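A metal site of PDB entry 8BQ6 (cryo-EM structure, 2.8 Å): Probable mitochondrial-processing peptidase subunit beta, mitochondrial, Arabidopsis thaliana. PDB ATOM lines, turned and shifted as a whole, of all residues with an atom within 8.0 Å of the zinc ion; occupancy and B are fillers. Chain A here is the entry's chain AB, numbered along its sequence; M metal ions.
Three residues have an atom within 4 Å of the zinc ion: His 141, His 145 and Glu 221.
ND1 of His 145 is in hydrogen-bond range of OE1 of Glu 214, 3.2 Å away.
NE2 of His 145 is bound to the zinc ion (2.3 Å).
A ring nitrogen (NE2) of His 141 is bound to the zinc ion.
OE2 of Glu 221 is bound to the zinc ion (2.3 Å).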
ATOM      1  N   HIS A 141     -18.942   4.611 -21.534  1.00  0.00           N
ATOM      2  CA  HIS A 141     -19.147   5.966 -22.042  1.00  0.00           C
ATOM      3  C   HIS A 141     -18.759   6.060 -23.508  1.00  0.00           C
ATOM      4  O   HIS A 141     -19.430   6.754 -24.287  1.00  0.00           O
ATOM      5  CB  HIS A 141     -18.355   6.974 -21.209  1.00  0.00           C
ATOM      6  CG  HIS A 141     -18.467   8.377 -21.719  1.00  0.00           C
ATOM      7  ND1 HIS A 141     -17.400   9.082 -22.221  1.00  0.00           N
ATOM      8  CD2 HIS A 141     -19.545   9.197 -21.822  1.00  0.00           C
ATOM      9  CE1 HIS A 141     -17.803  10.279 -22.606  1.00  0.00           C
ATOM     10  NE2 HIS A 141     -19.099  10.375 -22.377  1.00  0.00           N
ATOM     11  N   PHE A 142     -17.686   5.378 -23.911  1.00  0.00           N
ATOM     12  CA  PHE A 142     -17.301   5.359 -25.312  1.00  0.00           C
ATOM     13  C   PHE A 142     -18.369   4.699 -26.167  1.00  0.00           C
ATOM     14  O   PHE A 142     -18.667   5.164 -27.274  1.00  0.00           O
ATOM     15  CB  PHE A 142     -15.966   4.632 -25.473  1.00  0.00           C
ATOM     16  CG  PHE A 142     -15.124   5.160 -26.586  1.00  0.00           C
ATOM     17  CD1 PHE A 142     -15.453   4.900 -27.910  1.00  0.00           C
ATOM     18  CD2 PHE A 142     -14.005   5.931 -26.327  1.00  0.00           C
ATOM     19  CE1 PHE A 142     -14.682   5.389 -28.934  1.00  0.00           C
ATOM     20  CE2 PHE A 142     -13.235   6.420 -27.350  1.00  0.00           C
ATOM     21  CZ  PHE A 142     -13.567   6.148 -28.653  1.00  0.00           C
ATOM     22  N   GLU A 144     -21.479   4.673 -25.422  1.00  0.00           N
ATOM     23  CA  GLU A 144     -22.623   5.572 -25.424  1.00  0.00           C
ATOM     24  C   GLU A 144     -22.567   6.549 -26.595  1.00  0.00           C
ATOM     25  O   GLU A 144     -23.605   6.929 -27.140  1.00  0.00           O
ATOM     26  CB  GLU A 144     -22.696   6.326 -24.097  1.00  0.00           C
ATOM     27  CG  GLU A 144     -24.017   7.007 -23.845  1.00  0.00           C
ATOM     28  CD  GLU A 144     -23.845   8.363 -23.201  1.00  0.00           C
ATOM     29  OE1 GLU A 144     -23.558   9.340 -23.934  1.00  0.00           O
ATOM     30  OE2 GLU A 144     -24.018   8.469 -21.972  1.00  0.00           O
ATOM     31  N   HIS A 145     -21.361   6.967 -26.975  1.00  0.00           N
ATOM     32  CA  HIS A 145     -21.215   7.904 -28.079  1.00  0.00           C
ATOM     33  C   HIS A 145     -21.347   7.202 -29.425  1.00  0.00           C
ATOM     34  O   HIS A 145     -21.771   7.816 -30.412  1.00  0.00           O
ATOM     35  CB  HIS A 145     -19.868   8.614 -27.993  1.00  0.00           C
ATOM     36  CG  HIS A 145     -19.823   9.693 -26.961  1.00  0.00           C
ATOM     37  ND1 HIS A 145     -19.656  11.030 -27.288  1.00  0.00           N
ATOM     38  CD2 HIS A 145     -19.920   9.648 -25.618  1.00  0.00           C
ATOM     39  CE1 HIS A 145     -19.651  11.743 -26.185  1.00  0.00           C
ATOM     40  NE2 HIS A 145     -19.814  10.941 -25.153  1.00  0.00           N
ATOM     41  N   THR A 174     -25.638   6.649 -19.559  1.00  0.00           N
ATOM     42  CA  THR A 174     -24.899   5.627 -18.842  1.00  0.00           C
ATOM     43  C   THR A 174     -24.486   6.141 -17.467  1.00  0.00           C
ATOM     44  O   THR A 174     -24.189   7.324 -17.301  1.00  0.00           O
ATOM     45  CB  THR A 174     -23.655   5.174 -19.609  1.00  0.00           C
ATOM     46  OG1 THR A 174     -22.939   4.202 -18.841  1.00  0.00           O
ATOM     47  CG2 THR A 174     -22.733   6.351 -19.912  1.00  0.00           C
ATOM     48  N   GLU A 214     -14.731  10.154 -32.651  1.00  0.00           N
ATOM     49  CA  GLU A 214     -15.264  10.334 -31.309  1.00  0.00           C
ATOM     50  C   GLU A 214     -14.162  10.246 -30.262  1.00  0.00           C
ATOM     51  O   GLU A 214     -14.372  10.663 -29.113  1.00  0.00           O
ATOM     52  CB  GLU A 214     -16.341   9.296 -31.022  1.00  0.00           C
ATOM     53  CG  GLU A 214     -17.733   9.615 -31.591  1.00  0.00           C
ATOM     54  CD  GLU A 214     -18.253  11.001 -31.240  1.00  0.00           C
ATOM     55  OE1 GLU A 214     -19.246  11.094 -30.480  1.00  0.00           O
ATOM     56  OE2 GLU A 214     -17.715  12.008 -31.741  1.00  0.00           O
ATOM     57  N   VAL A 217     -13.359  13.726 -29.580  1.00  0.00           N
ATOM     58  CA  VAL A 217     -14.552  14.418 -29.000  1.00  0.00           C
ATOM     59  C   VAL A 217     -14.618  14.103 -27.497  1.00  0.00           C
ATOM     60  O   VAL A 217     -14.870  15.025 -26.712  1.00  0.00           O
ATOM     61  CB  VAL A 217     -15.844  14.030 -29.751  1.00  0.00           C
ATOM     62  CG1 VAL A 217     -17.080  14.037 -28.864  1.00  0.00           C
ATOM     63  CG2 VAL A 217     -16.053  14.916 -30.965  1.00  0.00           C
ATOM     64  N   ILE A 218     -14.354  12.840 -27.132  1.00  0.00           N
ATOM     65  CA  ILE A 218     -14.387  12.432 -25.697  1.00  0.00           C
ATOM     66  C   ILE A 218     -13.136  12.996 -25.004  1.00  0.00           C
ATOM     67  O   ILE A 218     -13.260  13.431 -23.850  1.00  0.00           O
ATOM     68  CB  ILE A 218     -14.550  10.910 -25.579  1.00  0.00           C
ATOM     69  CG1 ILE A 218     -15.933  10.471 -26.068  1.00  0.00           C
ATOM     70  CG2 ILE A 218     -14.271  10.410 -24.167  1.00  0.00           C
ATOM     71  CD1 ILE A 218     -16.018   9.021 -26.441  1.00  0.00           C
ATOM     72  N   GLU A 221     -13.984  16.525 -24.109  1.00  0.00           N
ATOM     73  CA  GLU A 221     -14.815  16.517 -22.877  1.00  0.00           C
ATOM     74  C   GLU A 221     -13.905  16.396 -21.658  1.00  0.00           C
ATOM     75  O   GLU A 221     -14.036  17.254 -20.780  1.00  0.00           O
ATOM     76  CB  GLU A 221     -15.767  15.321 -22.883  1.00  0.00           C
ATOM     77  CG  GLU A 221     -16.959  15.465 -23.812  1.00  0.00           C
ATOM     78  CD  GLU A 221     -17.860  14.240 -23.778  1.00  0.00           C
ATOM     79  OE1 GLU A 221     -17.448  13.212 -24.348  1.00  0.00           O
ATOM     80  OE2 GLU A 221     -18.947  14.318 -23.194  1.00  0.00           O
ATOM     81  N   MET A 222     -13.031  15.391 -21.620  1.00  0.00           N
ATOM     82  CA  MET A 222     -12.092  15.177 -20.493  1.00  0.00           C
ATOM     83  C   MET A 222     -11.276  16.440 -20.174  1.00  0.00           C
ATOM     84  O   MET A 222     -10.915  16.628 -19.009  1.00  0.00           O
ATOM     85  CB  MET A 222     -11.114  14.056 -20.845  1.00  0.00           C
ATOM     86  CG  MET A 222     -11.738  12.692 -20.978  1.00  0.00           C
ATOM     87  SD  MET A 222     -10.488  11.409 -20.785  1.00  0.00           S
ATOM     88  CE  MET A 222      -9.635  12.026 -19.338  1.00  0.00           C
ATOM     89  N   ILE A 251     -17.182   7.679 -14.750  1.00  0.00           N
ATOM     90  CA  ILE A 251     -17.815   7.174 -15.963  1.00  0.00           C
ATOM     91  C   ILE A 251     -16.929   7.470 -17.173  1.00  0.00           C
ATOM     92  O   ILE A 251     -16.742   6.612 -18.043  1.00  0.00           O
ATOM     93  CB  ILE A 251     -19.220   7.777 -16.126  1.00  0.00           C
ATOM     94  CG1 ILE A 251     -20.212   7.079 -15.197  1.00  0.00           C
ATOM     95  CG2 ILE A 251     -19.689   7.678 -17.555  1.00  0.00           C
ATOM     96  CD1 ILE A 251     -21.272   7.992 -14.646  1.00  0.00           C
ATOM     97  N   LEU A 252     -16.346   8.671 -17.237  1.00  0.00           N
ATOM     98  CA  LEU A 252     -15.556   9.071 -18.388  1.00  0.00           C
ATOM     99  C   LEU A 252     -14.318   8.196 -18.569  1.00  0.00           C
ATOM    100  O   LEU A 252     -14.020   7.755 -19.685  1.00  0.00           O
ATOM    101  CB  LEU A 252     -15.140  10.533 -18.251  1.00  0.00           C
ATOM    102  CG  LEU A 252     -16.124  11.610 -18.721  1.00  0.00           C
ATOM    103  CD1 LEU A 252     -17.370  11.596 -17.857  1.00  0.00           C
ATOM    104  CD2 LEU A 252     -15.486  12.982 -18.727  1.00  0.00           C
HETATM  105 ZN    ZN M   1     -20.013  12.276 -23.295  1.00  0.00          ZN
